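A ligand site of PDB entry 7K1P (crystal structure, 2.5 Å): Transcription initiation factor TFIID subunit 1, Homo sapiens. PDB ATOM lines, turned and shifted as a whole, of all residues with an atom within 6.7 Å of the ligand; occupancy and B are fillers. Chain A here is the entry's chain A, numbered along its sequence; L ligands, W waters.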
ATOM      1  N   TRP A  28     -28.234   2.567  10.474  1.00  0.00           N
ATOM      2  CA  TRP A  28     -28.930   1.584  11.302  1.00  0.00           C
ATOM      3  C   TRP A  28     -28.047   0.789  12.267  1.00  0.00           C
ATOM      4  O   TRP A  28     -28.578   0.390  13.323  1.00  0.00           O
ATOM      5  CB  TRP A  28     -29.732   0.624  10.403  1.00  0.00           C
ATOM      6  CG  TRP A  28     -28.902  -0.245   9.502  1.00  0.00           C
ATOM      7  CD1 TRP A  28     -28.589  -0.012   8.194  1.00  0.00           C
ATOM      8  CD2 TRP A  28     -28.288  -1.500   9.852  1.00  0.00           C
ATOM      9  NE1 TRP A  28     -27.820  -1.038   7.709  1.00  0.00           N
ATOM     10  CE2 TRP A  28     -27.610  -1.956   8.700  1.00  0.00           C
ATOM     11  CE3 TRP A  28     -28.234  -2.267  11.016  1.00  0.00           C
ATOM     12  CZ2 TRP A  28     -26.895  -3.161   8.684  1.00  0.00           C
ATOM     13  CZ3 TRP A  28     -27.513  -3.460  11.000  1.00  0.00           C
ATOM     14  CH2 TRP A  28     -26.855  -3.897   9.836  1.00  0.00           C
ATOM     15  N   PRO A  29     -26.760   0.516  12.005  1.00  0.00           N
ATOM     16  CA  PRO A  29     -25.973  -0.167  13.043  1.00  0.00           C
ATOM     17  C   PRO A  29     -25.837   0.633  14.334  1.00  0.00           C
ATOM     18  O   PRO A  29     -25.479   0.058  15.369  1.00  0.00           O
ATOM     19  CB  PRO A  29     -24.603  -0.372  12.372  1.00  0.00           C
ATOM     20  CG  PRO A  29     -24.883  -0.329  10.925  1.00  0.00           C
ATOM     21  CD  PRO A  29     -25.973   0.701  10.779  1.00  0.00           C
ATOM     22  N   PHE A  30     -26.114   1.923  14.304  1.00  0.00           N
ATOM     23  CA  PHE A  30     -26.016   2.763  15.478  1.00  0.00           C
ATOM     24  C   PHE A  30     -27.350   2.981  16.171  1.00  0.00           C
ATOM     25  O   PHE A  30     -27.391   3.651  17.212  1.00  0.00           O
ATOM     26  CB  PHE A  30     -25.393   4.109  15.094  1.00  0.00           C
ATOM     27  CG  PHE A  30     -23.993   3.979  14.534  1.00  0.00           C
ATOM     28  CD1 PHE A  30     -22.921   3.805  15.382  1.00  0.00           C
ATOM     29  CD2 PHE A  30     -23.777   3.995  13.168  1.00  0.00           C
ATOM     30  CE1 PHE A  30     -21.631   3.661  14.882  1.00  0.00           C
ATOM     31  CE2 PHE A  30     -22.492   3.854  12.654  1.00  0.00           C
ATOM     32  CZ  PHE A  30     -21.418   3.694  13.520  1.00  0.00           C
ATOM     33  N   HIS A  31     -28.435   2.417  15.642  1.00  0.00           N
ATOM     34  CA  HIS A  31     -29.762   2.636  16.229  1.00  0.00           C
ATOM     35  C   HIS A  31     -29.989   1.833  17.492  1.00  0.00           C
ATOM     36  O   HIS A  31     -30.902   2.145  18.258  1.00  0.00           O
ATOM     37  CB  HIS A  31     -30.852   2.296  15.212  1.00  0.00           C
ATOM     38  CG  HIS A  31     -30.856   3.167  13.993  1.00  0.00           C
ATOM     39  ND1 HIS A  31     -31.865   3.144  13.058  1.00  0.00           N
ATOM     40  CD2 HIS A  31     -29.959   4.082  13.557  1.00  0.00           C
ATOM     41  CE1 HIS A  31     -31.594   4.013  12.102  1.00  0.00           C
ATOM     42  NE2 HIS A  31     -30.448   4.593  12.376  1.00  0.00           N
ATOM     43  N   HIS A  32     -29.199   0.797  17.741  1.00  0.00           N
ATOM     44  CA  HIS A  32     -29.420  -0.089  18.874  1.00  0.00           C
ATOM     45  C   HIS A  32     -28.070  -0.543  19.413  1.00  0.00           C
ATOM     46  O   HIS A  32     -27.056  -0.422  18.731  1.00  0.00           O
ATOM     47  CB  HIS A  32     -30.282  -1.289  18.464  1.00  0.00           C
ATOM     48  CG  HIS A  32     -31.609  -0.907  17.889  1.00  0.00           C
ATOM     49  ND1 HIS A  32     -32.663  -0.490  18.680  1.00  0.00           N
ATOM     50  CD2 HIS A  32     -32.040  -0.857  16.616  1.00  0.00           C
ATOM     51  CE1 HIS A  32     -33.697  -0.212  17.900  1.00  0.00           C
ATOM     52  NE2 HIS A  32     -33.344  -0.423  16.645  1.00  0.00           N
ATOM     53  N   PRO A  33     -28.030  -1.040  20.648  1.00  0.00           N
ATOM     54  CA  PRO A  33     -26.766  -1.540  21.197  1.00  0.00           C
ATOM     55  C   PRO A  33     -26.147  -2.558  20.255  1.00  0.00           C
ATOM     56  O   PRO A  33     -26.852  -3.318  19.584  1.00  0.00           O
ATOM     57  CB  PRO A  33     -27.168  -2.171  22.530  1.00  0.00           C
ATOM     58  CG  PRO A  33     -28.419  -1.422  22.933  1.00  0.00           C
ATOM     59  CD  PRO A  33     -29.129  -1.075  21.643  1.00  0.00           C
ATOM     60  N   VAL A  34     -24.816  -2.556  20.175  1.00  0.00           N
ATOM     61  CA  VAL A  34     -24.119  -3.548  19.373  1.00  0.00           C
ATOM     62  C   VAL A  34     -24.551  -4.940  19.826  1.00  0.00           C
ATOM     63  O   VAL A  34     -24.588  -5.220  21.029  1.00  0.00           O
ATOM     64  CB  VAL A  34     -22.598  -3.363  19.482  1.00  0.00           C
ATOM     65  CG1 VAL A  34     -21.865  -4.608  19.010  1.00  0.00           C
ATOM     66  CG2 VAL A  34     -22.149  -2.147  18.675  1.00  0.00           C
ATOM     67  N   ASN A  35     -24.906  -5.788  18.869  1.00  0.00           N
ATOM     68  CA  ASN A  35     -25.293  -7.163  19.177  1.00  0.00           C
ATOM     69  C   ASN A  35     -24.036  -8.005  19.295  1.00  0.00           C
ATOM     70  O   ASN A  35     -23.305  -8.182  18.316  1.00  0.00           O
ATOM     71  CB  ASN A  35     -26.222  -7.709  18.096  1.00  0.00           C
ATOM     72  CG  ASN A  35     -26.848  -9.039  18.484  1.00  0.00           C
ATOM     73  OD1 ASN A  35     -26.408  -9.695  19.434  1.00  0.00           O
ATOM     74  ND2 ASN A  35     -27.866  -9.443  17.733  1.00  0.00           N
ATOM     75  N   LYS A  36     -23.778  -8.533  20.497  1.00  0.00           N
ATOM     76  CA  LYS A  36     -22.592  -9.354  20.707  1.00  0.00           C
ATOM     77  C   LYS A  36     -22.573 -10.568  19.793  1.00  0.00           C
ATOM     78  O   LYS A  36     -21.491 -11.095  19.506  1.00  0.00           O
ATOM     79  CB  LYS A  36     -22.506  -9.769  22.177  1.00  0.00           C
ATOM     80  CG  LYS A  36     -21.145 -10.300  22.593  1.00  0.00           C
ATOM     81  CD  LYS A  36     -20.971 -10.273  24.107  1.00  0.00           C
ATOM     82  CE  LYS A  36     -21.999 -11.154  24.798  1.00  0.00           C
ATOM     83  NZ  LYS A  36     -21.866 -12.582  24.402  1.00  0.00           N
ATOM     84  N   PHE A  38     -22.980 -10.668  16.670  1.00  0.00           N
ATOM     85  CA  PHE A  38     -22.289 -10.312  15.445  1.00  0.00           C
ATOM     86  C   PHE A  38     -20.900  -9.742  15.667  1.00  0.00           C
ATOM     87  O   PHE A  38     -20.080  -9.808  14.759  1.00  0.00           O
ATOM     88  CB  PHE A  38     -23.114  -9.279  14.652  1.00  0.00           C
ATOM     89  CG  PHE A  38     -24.333  -9.845  14.020  1.00  0.00           C
ATOM     90  CD1 PHE A  38     -25.488 -10.043  14.759  1.00  0.00           C
ATOM     91  CD2 PHE A  38     -24.340 -10.178  12.668  1.00  0.00           C
ATOM     92  CE1 PHE A  38     -26.626 -10.571  14.171  1.00  0.00           C
ATOM     93  CE2 PHE A  38     -25.477 -10.691  12.067  1.00  0.00           C
ATOM     94  CZ  PHE A  38     -26.628 -10.899  12.826  1.00  0.00           C
ATOM     95  N   VAL A  39     -20.644  -9.164  16.835  1.00  0.00           N
ATOM     96  CA  VAL A  39     -19.359  -8.543  17.150  1.00  0.00           C
ATOM     97  C   VAL A  39     -18.876  -9.128  18.462  1.00  0.00           C
ATOM     98  O   VAL A  39     -19.022  -8.496  19.519  1.00  0.00           O
ATOM     99  CB  VAL A  39     -19.486  -7.007  17.221  1.00  0.00           C
ATOM    100  CG1 VAL A  39     -18.135  -6.354  17.095  1.00  0.00           C
ATOM    101  CG2 VAL A  39     -20.440  -6.485  16.149  1.00  0.00           C
ATOM    102  N   ASP A  41     -16.318  -9.499  20.294  1.00  0.00           N
ATOM    103  CA  ASP A  41     -15.383  -8.853  21.213  1.00  0.00           C
ATOM    104  C   ASP A  41     -15.684  -7.385  21.457  1.00  0.00           C
ATOM    105  O   ASP A  41     -14.829  -6.674  21.999  1.00  0.00           O
ATOM    106  CB  ASP A  41     -13.955  -9.007  20.692  1.00  0.00           C
ATOM    107  CG  ASP A  41     -13.715  -8.216  19.415  1.00  0.00           C
ATOM    108  OD1 ASP A  41     -14.697  -7.950  18.693  1.00  0.00           O
ATOM    109  OD2 ASP A  41     -12.540  -7.887  19.122  1.00  0.00           O
ATOM    110  N   TYR A  42     -16.880  -6.903  21.072  1.00  0.00           N
ATOM    111  CA  TYR A  42     -17.152  -5.473  21.195  1.00  0.00           C
ATOM    112  C   TYR A  42     -17.064  -5.011  22.638  1.00  0.00           C
ATOM    113  O   TYR A  42     -16.422  -4.007  22.947  1.00  0.00           O
ATOM    114  CB  TYR A  42     -18.518  -5.119  20.611  1.00  0.00           C
ATOM    115  CG  TYR A  42     -18.674  -3.635  20.425  1.00  0.00           C
ATOM    116  CD1 TYR A  42     -18.019  -2.983  19.396  1.00  0.00           C
ATOM    117  CD2 TYR A  42     -19.439  -2.858  21.304  1.00  0.00           C
ATOM    118  CE1 TYR A  42     -18.122  -1.618  19.216  1.00  0.00           C
ATOM    119  CE2 TYR A  42     -19.555  -1.480  21.138  1.00  0.00           C
ATOM    120  CZ  TYR A  42     -18.882  -0.874  20.087  1.00  0.00           C
ATOM    121  OH  TYR A  42     -18.963   0.482  19.884  1.00  0.00           O
ATOM    122  N   MET A  50     -22.384   2.864  23.645  1.00  0.00           N
ATOM    123  CA  MET A  50     -23.414   3.872  23.529  1.00  0.00           C
ATOM    124  C   MET A  50     -24.036   3.776  22.143  1.00  0.00           C
ATOM    125  O   MET A  50     -23.371   3.395  21.175  1.00  0.00           O
ATOM    126  CB  MET A  50     -22.858   5.280  23.777  1.00  0.00           C
ATOM    127  CG  MET A  50     -23.900   6.390  23.782  1.00  0.00           C
ATOM    128  SD  MET A  50     -25.294   6.089  24.896  1.00  0.00           S
ATOM    129  CE  MET A  50     -24.450   5.852  26.467  1.00  0.00           C
ATOM    130  N   ILE A  77     -20.555   7.851  20.872  1.00  0.00           N
ATOM    131  CA  ILE A  77     -20.822   6.890  19.792  1.00  0.00           C
ATOM    132  C   ILE A  77     -19.715   6.954  18.755  1.00  0.00           C
ATOM    133  O   ILE A  77     -19.245   5.920  18.260  1.00  0.00           O
ATOM    134  CB  ILE A  77     -22.206   7.169  19.161  1.00  0.00           C
ATOM    135  CG1 ILE A  77     -23.310   7.024  20.211  1.00  0.00           C
ATOM    136  CG2 ILE A  77     -22.443   6.222  17.992  1.00  0.00           C
ATOM    137  CD1 ILE A  77     -24.692   7.167  19.621  1.00  0.00           C
ATOM    138  N   ASN A  80     -16.279   5.580  20.179  1.00  0.00           N
ATOM    139  CA  ASN A  80     -16.279   4.134  20.276  1.00  0.00           C
ATOM    140  C   ASN A  80     -15.984   3.494  18.918  1.00  0.00           C
ATOM    141  O   ASN A  80     -15.166   2.566  18.812  1.00  0.00           O
ATOM    142  CB  ASN A  80     -17.619   3.634  20.825  1.00  0.00           C
ATOM    143  CG  ASN A  80     -17.757   3.873  22.307  1.00  0.00           C
ATOM    144  OD1 ASN A  80     -16.761   4.055  23.021  1.00  0.00           O
ATOM    145  ND2 ASN A  80     -18.985   3.847  22.802  1.00  0.00           N
ATOM    146  N   SER A  81     -16.639   3.999  17.860  1.00  0.00           N
ATOM    147  CA  SER A  81     -16.413   3.437  16.537  1.00  0.00           C
ATOM    148  C   SER A  81     -14.991   3.723  16.057  1.00  0.00           C
ATOM    149  O   SER A  81     -14.397   2.899  15.363  1.00  0.00           O
ATOM    150  CB  SER A  81     -17.430   4.008  15.546  1.00  0.00           C
ATOM    151  OG  SER A  81     -16.934   3.928  14.236  1.00  0.00           O
ATOM    152  N   TYR A  84     -12.997   1.057  17.908  1.00  0.00           N
ATOM    153  CA  TYR A  84     -13.211  -0.331  17.503  1.00  0.00           C
ATOM    154  C   TYR A  84     -12.921  -0.540  16.019  1.00  0.00           C
ATOM    155  O   TYR A  84     -12.331  -1.566  15.646  1.00  0.00           O
ATOM    156  CB  TYR A  84     -14.632  -0.789  17.822  1.00  0.00           C
ATOM    157  CG  TYR A  84     -14.781  -2.281  17.617  1.00  0.00           C
ATOM    158  CD1 TYR A  84     -14.269  -3.166  18.540  1.00  0.00           C
ATOM    159  CD2 TYR A  84     -15.380  -2.792  16.474  1.00  0.00           C
ATOM    160  CE1 TYR A  84     -14.358  -4.538  18.347  1.00  0.00           C
ATOM    161  CE2 TYR A  84     -15.491  -4.154  16.275  1.00  0.00           C
ATOM    162  CZ  TYR A  84     -14.977  -5.025  17.215  1.00  0.00           C
ATOM    163  OH  TYR A  84     -15.070  -6.388  17.034  1.00  0.00           O
ATOM    164  N   ASN A  85     -13.321   0.391  15.154  1.00  0.00           N
ATOM    165  CA  ASN A  85     -13.208   0.184  13.723  1.00  0.00           C
ATOM    166  C   ASN A  85     -12.020   0.901  13.096  1.00  0.00           C
ATOM    167  O   ASN A  85     -11.560   0.481  12.031  1.00  0.00           O
ATOM    168  CB  ASN A  85     -14.485   0.660  13.016  1.00  0.00           C
ATOM    169  CG  ASN A  85     -15.716  -0.069  13.512  1.00  0.00           C
ATOM    170  OD1 ASN A  85     -15.854  -1.278  13.335  1.00  0.00           O
ATOM    171  ND2 ASN A  85     -16.628   0.682  14.129  1.00  0.00           N
ATOM    172  N   SER A  89     -12.605   3.762   8.839  1.00  0.00           N
ATOM    173  CA  SER A  89     -13.622   2.754   8.557  1.00  0.00           C
ATOM    174  C   SER A  89     -14.947   3.407   8.183  1.00  0.00           C
ATOM    175  O   SER A  89     -15.266   4.521   8.612  1.00  0.00           O
ATOM    176  CB  SER A  89     -13.814   1.858   9.777  1.00  0.00           C
ATOM    177  OG  SER A  89     -15.132   1.357   9.840  1.00  0.00           O
ATOM    178  N   TYR A  91     -17.897   2.498   9.079  1.00  0.00           N
ATOM    179  CA  TYR A  91     -18.681   2.678  10.307  1.00  0.00           C
ATOM    180  C   TYR A  91     -18.373   4.026  10.947  1.00  0.00           C
ATOM    181  O   TYR A  91     -19.281   4.771  11.337  1.00  0.00           O
ATOM    182  CB  TYR A  91     -18.375   1.544  11.288  1.00  0.00           C
ATOM    183  CG  TYR A  91     -18.944   0.204  10.900  1.00  0.00           C
ATOM    184  CD1 TYR A  91     -20.302  -0.060  11.005  1.00  0.00           C
ATOM    185  CD2 TYR A  91     -18.119  -0.802  10.417  1.00  0.00           C
ATOM    186  CE1 TYR A  91     -20.823  -1.299  10.651  1.00  0.00           C
ATOM    187  CE2 TYR A  91     -18.630  -2.037  10.054  1.00  0.00           C
ATOM    188  CZ  TYR A  91     -19.981  -2.274  10.176  1.00  0.00           C
ATOM    189  OH  TYR A  91     -20.487  -3.504   9.821  1.00  0.00           O
HETATM  190  C1  LIG L   1     -22.892  -4.417  13.232  1.00  0.00           C
HETATM  191  N1  LIG L   1     -22.014  -2.505  14.238  1.00  0.00           N
HETATM  192  C2  LIG L   1     -19.424  -3.197  13.682  1.00  0.00           C
HETATM  193  C3  LIG L   1     -17.426  -4.459  12.591  1.00  0.00           C
HETATM  194  C4  LIG L   1     -15.038  -6.237  13.243  1.00  0.00           C
HETATM  195  C5  LIG L   1     -20.486  -4.029  13.289  1.00  0.00           C
HETATM  196  C6  LIG L   1     -22.200   0.272  15.817  1.00  0.00           C
HETATM  197  C7  LIG L   1     -23.869  -6.242  12.016  1.00  0.00           C
HETATM  198  C8  LIG L   1     -26.331  -6.822  12.253  1.00  0.00           C
HETATM  199  C9  LIG L   1     -25.109  -5.976  12.593  1.00  0.00           C
HETATM  200  C10 LIG L   1     -25.241  -4.951  13.496  1.00  0.00           C
HETATM  201  N2  LIG L   1     -26.540  -4.689  14.075  1.00  0.00           N
HETATM  202  S1  LIG L   1     -26.725  -4.447  15.759  1.00  0.00           S
HETATM  203  C11 LIG L   1     -27.093  -2.701  16.076  1.00  0.00           C
HETATM  204  O1  LIG L   1     -25.530  -4.892  16.489  1.00  0.00           O
HETATM  205  O2  LIG L   1     -27.765  -5.331  16.303  1.00  0.00           O
HETATM  206  C12 LIG L   1     -24.133  -4.160  13.815  1.00  0.00           C
HETATM  207  C13 LIG L   1     -21.800  -3.636  13.583  1.00  0.00           C
HETATM  208  N3  LIG L   1     -20.970  -1.672  14.644  1.00  0.00           N
HETATM  209  C14 LIG L   1     -19.729  -1.993  14.378  1.00  0.00           C
HETATM  210  N4  LIG L   1     -18.010  -3.453  13.460  1.00  0.00           N
HETATM  211  O3  LIG L   1     -16.075  -4.327  12.260  1.00  0.00           O
HETATM  212  C15 LIG L   1     -15.416  -5.529  11.939  1.00  0.00           C
HETATM  213  O4  LIG L   1     -18.059  -5.368  12.192  1.00  0.00           O
HETATM  214  N5  LIG L   1     -18.920  -1.031  14.870  1.00  0.00           N
HETATM  215  N6  LIG L   1     -19.709  -0.087  15.459  1.00  0.00           N
HETATM  216  C16 LIG L   1     -20.965  -0.480  15.314  1.00  0.00           C
HETATM  217  C17 LIG L   1     -22.768  -5.463  12.334  1.00  0.00           C
HETATM  218  O   HOH W   1     -24.594   0.610  17.935  1.00  0.00           O
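Trp 28 touches the ligand. Pro 29 touches the ligand. Phe 30 touches the ligand (CE1 to C6, 3.6 Å). O of His 32 touches C11 of the ligand (3.5 Å). Pro 33 touches the ligand (O to C11, 3.6 Å). Val 34 touches the ligand. Phe 38 touches the ligand (CD2 to C8, 3.9 Å). Val 39 touches the ligand (CG2 to C5, 3.8 Å). CE2 of Tyr 84 touches C4 of the ligand, at 3.7 Å. Tyr 91 touches the ligand (OH to C5, 3.5 Å). Hydrophobic or aromatic side chains within 4 Å of the ligand: Trp 28, Pro 29, Phe 30, Val 34, Phe 38, Val 39, Tyr 84 and Tyr 91. Of the 21 residues printed, 12 come within 4 Å of the ligand.
ND2 of Asn 85 sits at hydrogen-bond distance from OG of Ser 81, 3.3 Å away. The backbone NH of Tyr 91 sits at hydrogen-bond distance from the side-chain hydroxyl of Ser 89, 3.1 Å away.
The backbone NH (N) of Asn 35 lies within hydrogen-bond range of an oxygen (O1) of the ligand. The side-chain amide nitrogen of Asn 85 lies within hydrogen-bond range of a nitrogen (N5) of the ligand (3.0 Å).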
